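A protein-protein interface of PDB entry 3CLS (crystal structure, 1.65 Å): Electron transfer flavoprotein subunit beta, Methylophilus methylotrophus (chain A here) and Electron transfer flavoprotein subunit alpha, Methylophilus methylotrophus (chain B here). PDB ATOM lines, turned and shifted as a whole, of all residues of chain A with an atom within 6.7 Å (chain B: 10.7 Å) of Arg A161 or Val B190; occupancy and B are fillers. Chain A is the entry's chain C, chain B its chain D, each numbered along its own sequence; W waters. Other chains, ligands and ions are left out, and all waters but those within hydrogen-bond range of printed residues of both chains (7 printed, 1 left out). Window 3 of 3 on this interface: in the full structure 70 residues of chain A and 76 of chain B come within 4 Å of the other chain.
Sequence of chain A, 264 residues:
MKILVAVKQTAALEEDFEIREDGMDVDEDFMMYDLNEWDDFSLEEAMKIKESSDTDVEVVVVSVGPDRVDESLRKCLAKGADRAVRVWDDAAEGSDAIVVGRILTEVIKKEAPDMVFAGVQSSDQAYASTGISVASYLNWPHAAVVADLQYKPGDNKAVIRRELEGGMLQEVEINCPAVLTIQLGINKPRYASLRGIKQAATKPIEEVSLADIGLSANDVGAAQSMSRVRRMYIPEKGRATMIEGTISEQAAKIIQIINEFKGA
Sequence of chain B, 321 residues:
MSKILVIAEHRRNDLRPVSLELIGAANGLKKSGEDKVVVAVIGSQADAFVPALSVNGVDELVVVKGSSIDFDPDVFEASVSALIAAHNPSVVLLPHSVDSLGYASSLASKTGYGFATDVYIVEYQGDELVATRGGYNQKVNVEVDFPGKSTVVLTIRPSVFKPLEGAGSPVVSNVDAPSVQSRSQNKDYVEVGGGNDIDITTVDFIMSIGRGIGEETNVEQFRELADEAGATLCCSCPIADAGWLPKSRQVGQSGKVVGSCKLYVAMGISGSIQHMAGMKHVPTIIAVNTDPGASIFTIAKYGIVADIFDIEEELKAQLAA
Hydrophobic or aromatic side chains of chain B that line the printed part of chain A: Val B98, Tyr B189, Val B190 and Val B192.
Of the 18 printed residues of chain A, 10 touch a printed residue of chain B.
Printed residues of chain A that touch a printed residue of chain B: Val A145, Arg A161, Arg A162, Glu A163, Gly A167, Met A168, Leu A169, Gln A170, Glu A171 and Val A172.
Hydrophobic or aromatic side chains of chain A within 4 Å of the printed part of chain B: Val A145, Met A168, Leu A169 and Val A172.
N of Glu A163 sits at hydrogen-bond distance from O of Val A145 (2.9 Å).
N of Arg A161 is in hydrogen-bond range of O of Asp A148 (3.0 Å).
OH of Tyr B189 is in hydrogen-bond range of OD2 of Asp B70, 2.6 Å away.
Water W4 lies within hydrogen-bond range of OD2 of Asp B188 (2.6 Å) and OE1 of Glu A171 (3.2 Å).
Water W3 lies within hydrogen-bond range of the backbone carbonyl oxygen (O) of Met A168 (3.0 Å), the backbone carbonyl oxygen (O) of Ser B254 (3.1 Å) and the backbone NH (N) of Gly A167 (3.5 Å).
Of chain B, only Val B190 (3.7 Å) comes within 4 Å of Arg A161.
Val B190 touches four residues of chain A.
Asp A148 touches none of the printed residues of chain B.
Met A168 touches just these residues of chain B: Arg B12 (3.2 Å) and Val B190 (3.5 Å).
Of chain B, only Asn B186 (3.8 Å), Lys B187 (2.8 Å), Asp B188 (2.8 Å) and Val B190 (3.97 Å) come within 4 Å of Glu A171.
Printed residues of chain A within 4 Å of Asp B188: Gln A170 (3.6 Å) and Glu A171 (2.8 Å).
Printed residues of chain A within 4 Å of Lys B256: Gly A167.
The nearest printed residue of chain A that does not touch Asn B186 is Arg A162 (5.6 Å).
The side-chain carboxylate (OD1) of Asp B99 is in salt-bridge range of the guanidinium group (NH1) of Arg A162 (2.8 Å).
OE1 of Glu A163 sits close to OG of Ser B254 (3.3 Å).
N of Gly A167 sits at hydrogen-bond distance from O of Ser B254, 2.9 Å away.
The backbone NH (N) of Leu A169 lies within hydrogen-bond range of the backbone carbonyl oxygen (O) of Val B190 (2.7 Å).
O of Glu A171 is in hydrogen-bond range of N of Lys B187, at 2.8 Å.
The backbone NH (N) of Glu A171 is in hydrogen-bond range of the backbone carbonyl oxygen (O) of Asp B188 (2.8 Å).
Arg A161 touches Val B190.
O of Glu A163 touches CG2 of Val B98 (3.5 Å).
Tyr B189 touches Leu A169.
Gln A170 touches Asp B188.
Gln A170 touches Tyr B189 (NE2 to OH, 3.5 Å).
O of Glu A171 touches C of Asn B186 (3.8 Å).
Val B190 touches Glu A171.
Ser B184 touches Val A172.
Val A172 touches Gln B185 (CA to O, 3.4 Å).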
ATOM      1  N   ALA A 144     -30.441  10.918  -3.455  1.00  0.00           N
ATOM      2  CA  ALA A 144     -29.195  11.348  -4.022  1.00  0.00           C
ATOM      3  C   ALA A 144     -27.936  10.787  -3.279  1.00  0.00           C
ATOM      4  O   ALA A 144     -27.852  10.812  -2.050  1.00  0.00           O
ATOM      5  CB  ALA A 144     -29.114  12.858  -4.122  1.00  0.00           C
ATOM      6  N   VAL A 145     -26.884  10.520  -4.070  1.00  0.00           N
ATOM      7  CA  VAL A 145     -25.543  10.125  -3.557  1.00  0.00           C
ATOM      8  C   VAL A 145     -25.571   8.695  -3.054  1.00  0.00           C
ATOM      9  O   VAL A 145     -25.194   8.375  -1.916  1.00  0.00           O
ATOM     10  CB  VAL A 145     -24.901  11.113  -2.588  1.00  0.00           C
ATOM     11  CG1 VAL A 145     -23.413  10.929  -2.558  1.00  0.00           C
ATOM     12  CG2 VAL A 145     -25.218  12.565  -2.971  1.00  0.00           C
ATOM     13  N   VAL A 146     -26.033   7.851  -3.933  1.00  0.00           N
ATOM     14  CA  VAL A 146     -26.262   6.425  -3.608  1.00  0.00           C
ATOM     15  C   VAL A 146     -24.953   5.641  -3.847  1.00  0.00           C
ATOM     16  O   VAL A 146     -24.471   5.586  -5.001  1.00  0.00           O
ATOM     17  CB  VAL A 146     -27.389   5.882  -4.446  1.00  0.00           C
ATOM     18  CG1 VAL A 146     -27.497   4.322  -4.304  1.00  0.00           C
ATOM     19  CG2 VAL A 146     -28.690   6.567  -4.118  1.00  0.00           C
ATOM     20  N   ALA A 147     -24.432   5.088  -2.752  1.00  0.00           N
ATOM     21  CA  ALA A 147     -23.202   4.272  -2.691  1.00  0.00           C
ATOM     22  C   ALA A 147     -23.467   2.758  -2.667  1.00  0.00           C
ATOM     23  O   ALA A 147     -22.530   1.990  -2.756  1.00  0.00           O
ATOM     24  CB  ALA A 147     -22.341   4.661  -1.497  1.00  0.00           C
ATOM     25  N   ASP A 148     -24.714   2.337  -2.538  1.00  0.00           N
ATOM     26  CA  ASP A 148     -25.065   0.942  -2.507  1.00  0.00           C
ATOM     27  C   ASP A 148     -26.542   0.839  -2.828  1.00  0.00           C
ATOM     28  O   ASP A 148     -27.348   1.703  -2.369  1.00  0.00           O
ATOM     29  CB  ASP A 148     -24.827   0.357  -1.102  1.00  0.00           C
ATOM     30  CG  ASP A 148     -24.932  -1.165  -1.089  1.00  0.00           C
ATOM     31  OD1 ASP A 148     -25.952  -1.712  -0.612  1.00  0.00           O
ATOM     32  OD2 ASP A 148     -23.999  -1.826  -1.599  1.00  0.00           O
ATOM     33  N   LEU A 149     -26.878  -0.222  -3.558  1.00  0.00           N
ATOM     34  CA  LEU A 149     -28.255  -0.469  -3.989  1.00  0.00           C
ATOM     35  C   LEU A 149     -28.599  -1.943  -3.849  1.00  0.00           C
ATOM     36  O   LEU A 149     -27.970  -2.786  -4.484  1.00  0.00           O
ATOM     37  CB  LEU A 149     -28.470  -0.037  -5.424  1.00  0.00           C
ATOM     38  CG  LEU A 149     -29.815  -0.351  -6.044  1.00  0.00           C
ATOM     39  CD1 LEU A 149     -30.966   0.259  -5.242  1.00  0.00           C
ATOM     40  CD2 LEU A 149     -29.843   0.173  -7.457  1.00  0.00           C
ATOM     41  N   GLN A 150     -29.586  -2.215  -3.026  1.00  0.00           N
ATOM     42  CA  GLN A 150     -30.139  -3.601  -2.864  1.00  0.00           C
ATOM     43  C   GLN A 150     -31.528  -3.570  -3.473  1.00  0.00           C
ATOM     44  O   GLN A 150     -32.438  -2.897  -2.946  1.00  0.00           O
ATOM     45  CB  GLN A 150     -30.186  -4.010  -1.414  1.00  0.00           C
ATOM     46  CG  GLN A 150     -28.862  -3.926  -0.708  1.00  0.00           C
ATOM     47  CD  GLN A 150     -27.856  -4.894  -1.236  1.00  0.00           C
ATOM     48  OE1 GLN A 150     -28.176  -6.058  -1.550  1.00  0.00           O
ATOM     49  NE2 GLN A 150     -26.598  -4.440  -1.323  1.00  0.00           N
ATOM     50  N   VAL A 159     -33.350  -0.929  -1.020  1.00  0.00           N
ATOM     51  CA  VAL A 159     -32.627  -0.371   0.106  1.00  0.00           C
ATOM     52  C   VAL A 159     -31.363   0.201  -0.437  1.00  0.00           C
ATOM     53  O   VAL A 159     -30.596  -0.516  -1.093  1.00  0.00           O
ATOM     54  CB  VAL A 159     -32.362  -1.398   1.221  1.00  0.00           C
ATOM     55  CG1 VAL A 159     -31.542  -0.791   2.374  1.00  0.00           C
ATOM     56  CG2 VAL A 159     -33.665  -1.906   1.789  1.00  0.00           C
ATOM     57  N   ILE A 160     -31.137   1.471  -0.128  1.00  0.00           N
ATOM     58  CA  ILE A 160     -29.955   2.186  -0.598  1.00  0.00           C
ATOM     59  C   ILE A 160     -29.152   2.658   0.562  1.00  0.00           C
ATOM     60  O   ILE A 160     -29.631   2.672   1.709  1.00  0.00           O
ATOM     61  CB  ILE A 160     -30.280   3.349  -1.589  1.00  0.00           C
ATOM     62  CG1 ILE A 160     -31.172   4.408  -0.936  1.00  0.00           C
ATOM     63  CG2 ILE A 160     -30.956   2.794  -2.891  1.00  0.00           C
ATOM     64  CD1 ILE A 160     -30.484   5.622  -0.465  1.00  0.00           C
ATOM     65  N   ARG A 161     -27.893   2.990   0.281  1.00  0.00           N
ATOM     66  CA  ARG A 161     -27.033   3.646   1.255  1.00  0.00           C
ATOM     67  C   ARG A 161     -26.554   4.921   0.667  1.00  0.00           C
ATOM     68  O   ARG A 161     -25.963   4.949  -0.448  1.00  0.00           O
ATOM     69  CB  ARG A 161     -25.834   2.815   1.700  1.00  0.00           C
ATOM     70  CG  ARG A 161     -26.221   1.678   2.587  1.00  0.00           C
ATOM     71  CD  ARG A 161     -25.080   0.794   2.991  1.00  0.00           C
ATOM     72  NE  ARG A 161     -25.614  -0.198   3.914  1.00  0.00           N
ATOM     73  CZ  ARG A 161     -24.873  -0.974   4.692  1.00  0.00           C
ATOM     74  NH1 ARG A 161     -23.555  -0.920   4.651  1.00  0.00           N
ATOM     75  NH2 ARG A 161     -25.474  -1.784   5.506  1.00  0.00           N
ATOM     76  N   ARG A 162     -26.896   6.008   1.328  1.00  0.00           N
ATOM     77  CA  ARG A 162     -26.371   7.304   0.856  1.00  0.00           C
ATOM     78  C   ARG A 162     -25.027   7.557   1.523  1.00  0.00           C
ATOM     79  O   ARG A 162     -24.787   7.173   2.683  1.00  0.00           O
ATOM     80  CB  ARG A 162     -27.274   8.535   0.994  1.00  0.00           C
ATOM     81  CG  ARG A 162     -28.514   8.489   1.548  1.00  0.00           C
ATOM     82  CD  ARG A 162     -29.158   9.894   1.582  1.00  0.00           C
ATOM     83  NE  ARG A 162     -29.333  10.328   2.952  1.00  0.00           N
ATOM     84  CZ  ARG A 162     -29.156  11.557   3.400  1.00  0.00           C
ATOM     85  NH1 ARG A 162     -28.779  12.539   2.566  1.00  0.00           N
ATOM     86  NH2 ARG A 162     -29.325  11.776   4.672  1.00  0.00           N
ATOM     87  N   GLU A 163     -24.107   8.117   0.733  1.00  0.00           N
ATOM     88  CA  GLU A 163     -22.752   8.411   1.200  1.00  0.00           C
ATOM     89  C   GLU A 163     -22.717   9.838   1.775  1.00  0.00           C
ATOM     90  O   GLU A 163     -22.860  10.814   1.037  1.00  0.00           O
ATOM     91  CB  GLU A 163     -21.747   8.217   0.066  1.00  0.00           C
ATOM     92  CG  GLU A 163     -20.305   8.527   0.493  1.00  0.00           C
ATOM     93  CD  GLU A 163     -19.375   8.617  -0.685  1.00  0.00           C
ATOM     94  OE1 GLU A 163     -19.162   9.734  -1.191  1.00  0.00           O
ATOM     95  OE2 GLU A 163     -18.908   7.545  -1.122  1.00  0.00           O
ATOM     96  N   GLY A 167     -17.360  10.219   6.372  1.00  0.00           N
ATOM     97  CA  GLY A 167     -17.124   8.795   6.484  1.00  0.00           C
ATOM     98  C   GLY A 167     -18.282   7.980   7.024  1.00  0.00           C
ATOM     99  O   GLY A 167     -18.081   6.879   7.611  1.00  0.00           O
ATOM    100  N   MET A 168     -19.493   8.451   6.836  1.00  0.00           N
ATOM    101  CA  MET A 168     -20.640   7.647   7.248  1.00  0.00           C
ATOM    102  C   MET A 168     -21.615   7.457   6.118  1.00  0.00           C
ATOM    103  O   MET A 168     -21.638   8.226   5.145  1.00  0.00           O
ATOM    104  CB  MET A 168     -21.293   8.196   8.509  1.00  0.00           C
ATOM    105  CG  MET A 168     -22.043   9.432   8.350  1.00  0.00           C
ATOM    106  SD  MET A 168     -22.608   9.880  10.022  1.00  0.00           S
ATOM    107  CE  MET A 168     -20.990  10.401  10.782  1.00  0.00           C
ATOM    108  N   LEU A 169     -22.386   6.387   6.235  1.00  0.00           N
ATOM    109  CA  LEU A 169     -23.439   6.103   5.315  1.00  0.00           C
ATOM    110  C   LEU A 169     -24.765   6.122   6.052  1.00  0.00           C
ATOM    111  O   LEU A 169     -24.831   5.978   7.293  1.00  0.00           O
ATOM    112  CB  LEU A 169     -23.237   4.721   4.673  1.00  0.00           C
ATOM    113  CG  LEU A 169     -21.815   4.365   4.194  1.00  0.00           C
ATOM    114  CD1 LEU A 169     -21.805   2.982   3.665  1.00  0.00           C
ATOM    115  CD2 LEU A 169     -21.475   5.310   3.093  1.00  0.00           C
ATOM    116  N   GLN A 170     -25.820   6.246   5.262  1.00  0.00           N
ATOM    117  CA  GLN A 170     -27.188   6.052   5.784  1.00  0.00           C
ATOM    118  C   GLN A 170     -27.998   5.091   4.912  1.00  0.00           C
ATOM    119  O   GLN A 170     -28.206   5.362   3.733  1.00  0.00           O
ATOM    120  CB  GLN A 170     -27.944   7.395   5.928  1.00  0.00           C
ATOM    121  CG  GLN A 170     -29.334   7.229   6.565  1.00  0.00           C
ATOM    122  CD  GLN A 170     -30.123   8.554   6.525  1.00  0.00           C
ATOM    123  OE1 GLN A 170     -30.101   9.254   5.496  1.00  0.00           O
ATOM    124  NE2 GLN A 170     -30.767   8.903   7.611  1.00  0.00           N
ATOM    125  N   GLU A 171     -28.528   4.018   5.508  1.00  0.00           N
ATOM    126  CA  GLU A 171     -29.461   3.162   4.834  1.00  0.00           C
ATOM    127  C   GLU A 171     -30.803   3.847   4.777  1.00  0.00           C
ATOM    128  O   GLU A 171     -31.255   4.418   5.774  1.00  0.00           O
ATOM    129  CB  GLU A 171     -29.638   1.839   5.538  1.00  0.00           C
ATOM    130  CG  GLU A 171     -28.424   1.037   5.661  1.00  0.00           C
ATOM    131  CD  GLU A 171     -28.760  -0.408   5.911  1.00  0.00           C
ATOM    132  OE1 GLU A 171     -29.341  -0.687   6.971  1.00  0.00           O
ATOM    133  OE2 GLU A 171     -28.505  -1.220   4.995  1.00  0.00           O
ATOM    134  N   VAL A 172     -31.427   3.756   3.607  1.00  0.00           N
ATOM    135  CA  VAL A 172     -32.767   4.312   3.369  1.00  0.00           C
ATOM    136  C   VAL A 172     -33.540   3.257   2.553  1.00  0.00           C
ATOM    137  O   VAL A 172     -33.016   2.787   1.528  1.00  0.00           O
ATOM    138  CB  VAL A 172     -32.681   5.594   2.550  1.00  0.00           C
ATOM    139  CG1 VAL A 172     -34.089   6.144   2.224  1.00  0.00           C
ATOM    140  CG2 VAL A 172     -31.774   6.643   3.208  1.00  0.00           C
ATOM    141  N   ARG B  11     -27.566  16.450  11.956  1.00  0.00           N
ATOM    142  CA  ARG B  11     -27.537  15.003  11.730  1.00  0.00           C
ATOM    143  C   ARG B  11     -27.091  14.364  13.020  1.00  0.00           C
ATOM    144  O   ARG B  11     -26.157  14.869  13.643  1.00  0.00           O
ATOM    145  CB  ARG B  11     -26.577  14.687  10.595  1.00  0.00           C
ATOM    146  CG  ARG B  11     -26.176  13.246  10.429  1.00  0.00           C
ATOM    147  CD  ARG B  11     -25.325  13.015   9.214  1.00  0.00           C
ATOM    148  NE  ARG B  11     -25.946  13.437   7.938  1.00  0.00           N
ATOM    149  CZ  ARG B  11     -25.389  14.146   6.967  1.00  0.00           C
ATOM    150  NH1 ARG B  11     -24.133  14.540   7.020  1.00  0.00           N
ATOM    151  NH2 ARG B  11     -26.131  14.456   5.904  1.00  0.00           N
ATOM    152  N   ARG B  12     -27.711  13.258  13.402  1.00  0.00           N
ATOM    153  CA  ARG B  12     -27.205  12.524  14.568  1.00  0.00           C
ATOM    154  C   ARG B  12     -27.047  13.417  15.803  1.00  0.00           C
ATOM    155  O   ARG B  12     -26.043  13.349  16.532  1.00  0.00           O
ATOM    156  CB  ARG B  12     -25.850  11.887  14.254  1.00  0.00           C
ATOM    157  CG  ARG B  12     -25.889  10.563  13.604  1.00  0.00           C
ATOM    158  CD  ARG B  12     -24.581   9.736  13.995  1.00  0.00           C
ATOM    159  NE  ARG B  12     -23.350  10.560  13.985  1.00  0.00           N
ATOM    160  CZ  ARG B  12     -22.105  10.069  13.907  1.00  0.00           C
ATOM    161  NH1 ARG B  12     -21.904   8.769  13.801  1.00  0.00           N
ATOM    162  NH2 ARG B  12     -21.049  10.880  13.934  1.00  0.00           N
ATOM    163  N   ASP B  70     -34.033  12.871  11.104  1.00  0.00           N
ATOM    164  CA  ASP B  70     -33.052  13.537  10.248  1.00  0.00           C
ATOM    165  C   ASP B  70     -33.580  13.684   8.804  1.00  0.00           C
ATOM    166  O   ASP B  70     -34.748  13.320   8.472  1.00  0.00           O
ATOM    167  CB  ASP B  70     -31.730  12.748  10.327  1.00  0.00           C
ATOM    168  CG  ASP B  70     -30.992  12.965  11.642  1.00  0.00           C
ATOM    169  OD1 ASP B  70     -31.426  13.894  12.364  1.00  0.00           O
ATOM    170  OD2 ASP B  70     -30.024  12.198  11.992  1.00  0.00           O
ATOM    171  N   VAL B  98     -24.764  16.873   0.975  1.00  0.00           N
ATOM    172  CA  VAL B  98     -25.398  15.639   0.521  1.00  0.00           C
ATOM    173  C   VAL B  98     -26.904  15.666   0.734  1.00  0.00           C
ATOM    174  O   VAL B  98     -27.679  15.319  -0.151  1.00  0.00           O
ATOM    175  CB  VAL B  98     -24.715  14.401   1.141  1.00  0.00           C
ATOM    176  CG1 VAL B  98     -25.490  13.181   0.821  1.00  0.00           C
ATOM    177  CG2 VAL B  98     -23.248  14.273   0.644  1.00  0.00           C
ATOM    178  N   ASP B  99     -27.337  16.170   1.881  1.00  0.00           N
ATOM    179  CA  ASP B  99     -28.771  16.281   2.147  1.00  0.00           C
ATOM    180  C   ASP B  99     -29.393  17.178   1.122  1.00  0.00           C
ATOM    181  O   ASP B  99     -30.399  16.848   0.472  1.00  0.00           O
ATOM    182  CB  ASP B  99     -29.014  16.882   3.508  1.00  0.00           C
ATOM    183  CG  ASP B  99     -28.849  15.903   4.641  1.00  0.00           C
ATOM    184  OD1 ASP B  99     -28.670  14.684   4.377  1.00  0.00           O
ATOM    185  OD2 ASP B  99     -28.918  16.394   5.812  1.00  0.00           O
ATOM    186  N   SER B 184     -39.937   7.332   1.242  1.00  0.00           N
ATOM    187  CA  SER B 184     -38.792   6.572   1.709  1.00  0.00           C
ATOM    188  C   SER B 184     -38.775   6.678   3.232  1.00  0.00           C
ATOM    189  O   SER B 184     -39.461   7.501   3.823  1.00  0.00           O
ATOM    190  CB  SER B 184     -37.466   7.089   1.065  1.00  0.00           C
ATOM    191  OG  SER B 184     -37.075   8.384   1.483  1.00  0.00           O
ATOM    192  N   GLN B 185     -38.023   5.781   3.846  1.00  0.00           N
ATOM    193  CA  GLN B 185     -37.859   5.693   5.303  1.00  0.00           C
ATOM    194  C   GLN B 185     -36.386   5.488   5.670  1.00  0.00           C
ATOM    195  O   GLN B 185     -35.701   4.632   5.107  1.00  0.00           O
ATOM    196  CB  GLN B 185     -38.693   4.549   5.882  1.00  0.00           C
ATOM    197  CG  GLN B 185     -38.280   4.191   7.279  1.00  0.00           C
ATOM    198  CD  GLN B 185     -38.764   5.171   8.333  1.00  0.00           C
ATOM    199  OE1 GLN B 185     -39.822   5.820   8.146  1.00  0.00           O
ATOM    200  NE2 GLN B 185     -38.012   5.271   9.473  1.00  0.00           N
ATOM    201  N   ASN B 186     -35.903   6.294   6.618  1.00  0.00           N
ATOM    202  CA  ASN B 186     -34.480   6.270   6.983  1.00  0.00           C
ATOM    203  C   ASN B 186     -34.295   5.083   7.917  1.00  0.00           C
ATOM    204  O   ASN B 186     -35.146   4.773   8.757  1.00  0.00           O
ATOM    205  CB  ASN B 186     -34.103   7.527   7.694  1.00  0.00           C
ATOM    206  CG  ASN B 186     -34.080   8.760   6.769  1.00  0.00           C
ATOM    207  OD1 ASN B 186     -33.968   8.621   5.520  1.00  0.00           O
ATOM    208  ND2 ASN B 186     -34.170   9.934   7.370  1.00  0.00           N
ATOM    209  N   LYS B 187     -33.202   4.376   7.721  1.00  0.00           N
ATOM    210  CA  LYS B 187     -32.851   3.225   8.503  1.00  0.00           C
ATOM    211  C   LYS B 187     -31.528   3.531   9.190  1.00  0.00           C
ATOM    212  O   LYS B 187     -31.315   4.655   9.594  1.00  0.00           O
ATOM    213  CB  LYS B 187     -32.896   1.989   7.659  1.00  0.00           C
ATOM    214  CG  LYS B 187     -34.231   1.723   6.987  1.00  0.00           C
ATOM    215  CD  LYS B 187     -35.303   1.388   8.008  1.00  0.00           C
ATOM    216  CE  LYS B 187     -36.592   1.097   7.339  1.00  0.00           C
ATOM    217  NZ  LYS B 187     -37.660   0.790   8.344  1.00  0.00           N
ATOM    218  N   ASP B 188     -30.677   2.539   9.405  1.00  0.00           N
ATOM    219  CA  ASP B 188     -29.460   2.731  10.171  1.00  0.00           C
ATOM    220  C   ASP B 188     -28.473   3.705   9.548  1.00  0.00           C
ATOM    221  O   ASP B 188     -28.270   3.719   8.321  1.00  0.00           O
ATOM    222  CB  ASP B 188     -28.739   1.389  10.374  1.00  0.00           C
ATOM    223  CG  ASP B 188     -29.453   0.441  11.363  1.00  0.00           C
ATOM    224  OD1 ASP B 188     -30.264   0.915  12.197  1.00  0.00           O
ATOM    225  OD2 ASP B 188     -29.215  -0.799  11.290  1.00  0.00           O
ATOM    226  N   TYR B 189     -27.802   4.494  10.384  1.00  0.00           N
ATOM    227  CA  TYR B 189     -26.503   5.034   9.941  1.00  0.00           C
ATOM    228  C   TYR B 189     -25.480   3.876  10.020  1.00  0.00           C
ATOM    229  O   TYR B 189     -25.572   2.965  10.861  1.00  0.00           O
ATOM    230  CB  TYR B 189     -26.030   6.208  10.809  1.00  0.00           C
ATOM    231  CG  TYR B 189     -26.834   7.465  10.644  1.00  0.00           C
ATOM    232  CD1 TYR B 189     -27.727   7.905  11.643  1.00  0.00           C
ATOM    233  CD2 TYR B 189     -26.788   8.182   9.458  1.00  0.00           C
ATOM    234  CE1 TYR B 189     -28.469   9.079  11.479  1.00  0.00           C
ATOM    235  CE2 TYR B 189     -27.544   9.329   9.273  1.00  0.00           C
ATOM    236  CZ  TYR B 189     -28.400   9.800  10.258  1.00  0.00           C
ATOM    237  OH  TYR B 189     -29.115  10.971   9.932  1.00  0.00           O
ATOM    238  N   VAL B 190     -24.468   3.958   9.151  1.00  0.00           N
ATOM    239  CA  VAL B 190     -23.446   2.931   9.054  1.00  0.00           C
ATOM    240  C   VAL B 190     -22.073   3.550   8.877  1.00  0.00           C
ATOM    241  O   VAL B 190     -21.890   4.527   8.097  1.00  0.00           O
ATOM    242  CB  VAL B 190     -23.706   1.982   7.846  1.00  0.00           C
ATOM    243  CG1 VAL B 190     -22.727   0.856   7.832  1.00  0.00           C
ATOM    244  CG2 VAL B 190     -25.156   1.428   7.873  1.00  0.00           C
ATOM    245  N   GLU B 191     -21.149   3.044   9.680  1.00  0.00           N
ATOM    246  CA  GLU B 191     -19.728   3.199   9.488  1.00  0.00           C
ATOM    247  C   GLU B 191     -19.212   1.848   8.989  1.00  0.00           C
ATOM    248  O   GLU B 191     -19.017   0.905   9.774  1.00  0.00           O
ATOM    249  CB  GLU B 191     -19.094   3.395  10.833  1.00  0.00           C
ATOM    250  CG  GLU B 191     -17.817   4.052  10.844  1.00  0.00           C
ATOM    251  CD  GLU B 191     -17.935   5.416  11.416  1.00  0.00           C
ATOM    252  OE1 GLU B 191     -19.054   5.830  11.798  1.00  0.00           O
ATOM    253  OE2 GLU B 191     -16.893   6.080  11.478  1.00  0.00           O
ATOM    254  N   VAL B 192     -19.015   1.725   7.695  1.00  0.00           N
ATOM    255  CA  VAL B 192     -18.492   0.468   7.116  1.00  0.00           C
ATOM    256  C   VAL B 192     -17.140  -0.057   7.626  1.00  0.00           C
ATOM    257  O   VAL B 192     -16.300   0.682   8.183  1.00  0.00           O
ATOM    258  CB  VAL B 192     -18.262   0.579   5.613  1.00  0.00           C
ATOM    259  CG1 VAL B 192     -19.499   1.114   4.911  1.00  0.00           C
ATOM    260  CG2 VAL B 192     -17.037   1.417   5.374  1.00  0.00           C
ATOM    261  N   GLY B 193     -16.923  -1.340   7.327  1.00  0.00           N
ATOM    262  CA  GLY B 193     -15.698  -2.069   7.690  1.00  0.00           C
ATOM    263  C   GLY B 193     -14.521  -1.393   7.021  1.00  0.00           C
ATOM    264  O   GLY B 193     -14.660  -0.435   6.275  1.00  0.00           O
ATOM    265  N   GLY B 194     -13.359  -1.896   7.309  1.00  0.00           N
ATOM    266  CA  GLY B 194     -12.168  -1.336   6.780  1.00  0.00           C
ATOM    267  C   GLY B 194     -11.395  -1.081   8.019  1.00  0.00           C
ATOM    268  O   GLY B 194     -11.984  -0.764   9.084  1.00  0.00           O
ATOM    269  N   LYS B 247     -10.747   3.075   3.615  1.00  0.00           N
ATOM    270  CA  LYS B 247     -11.514   4.319   3.639  1.00  0.00           C
ATOM    271  C   LYS B 247     -11.079   5.250   4.786  1.00  0.00           C
ATOM    272  O   LYS B 247     -11.134   6.485   4.641  1.00  0.00           O
ATOM    273  CB  LYS B 247     -13.033   4.026   3.692  1.00  0.00           C
ATOM    274  CG  LYS B 247     -13.652   3.554   2.375  1.00  0.00           C
ATOM    275  CD  LYS B 247     -13.680   4.699   1.411  1.00  0.00           C
ATOM    276  CE  LYS B 247     -14.629   4.536   0.238  1.00  0.00           C
ATOM    277  NZ  LYS B 247     -14.483   5.721  -0.678  1.00  0.00           N
ATOM    278  N   SER B 254     -16.346  13.362   1.831  1.00  0.00           N
ATOM    279  CA  SER B 254     -16.941  12.096   2.199  1.00  0.00           C
ATOM    280  C   SER B 254     -15.950  11.231   3.022  1.00  0.00           C
ATOM    281  O   SER B 254     -16.372  10.257   3.663  1.00  0.00           O
ATOM    282  CB  SER B 254     -17.450  11.408   0.927  1.00  0.00           C
ATOM    283  OG  SER B 254     -16.362  10.874   0.240  1.00  0.00           O
ATOM    284  N   LYS B 256     -12.285  12.058   5.610  1.00  0.00           N
ATOM    285  CA  LYS B 256     -12.018  12.869   6.788  1.00  0.00           C
ATOM    286  C   LYS B 256     -11.303  14.200   6.469  1.00  0.00           C
ATOM    287  O   LYS B 256     -10.649  14.356   5.429  1.00  0.00           O
ATOM    288  CB  LYS B 256     -11.234  12.039   7.831  1.00  0.00           C
ATOM    289  CG  LYS B 256     -11.536  10.516   7.810  1.00  0.00           C
ATOM    290  CD  LYS B 256     -13.039  10.144   8.023  1.00  0.00           C
ATOM    291  CE  LYS B 256     -13.366   8.646   7.600  1.00  0.00           C
ATOM    292  NZ  LYS B 256     -13.292   8.266   6.101  1.00  0.00           N
HETATM  293  O   HOH W   1     -28.768  12.539   7.730  1.00  0.00           O
HETATM  294  O   HOH W   2     -32.858  10.474   3.771  1.00  0.00           O
HETATM  295  O   HOH W   3     -18.968   8.629   3.752  1.00  0.00           O
HETATM  296  O   HOH W   4     -27.666  -1.855   9.441  1.00  0.00           O
HETATM  297  O   HOH W   5     -28.813  12.775  -0.394  1.00  0.00           O
HETATM  298  O   HOH W   6     -30.594   7.181  10.082  1.00  0.00           O
HETATM  299  O   HOH W   7     -18.470   4.081   6.585  1.00  0.00           O
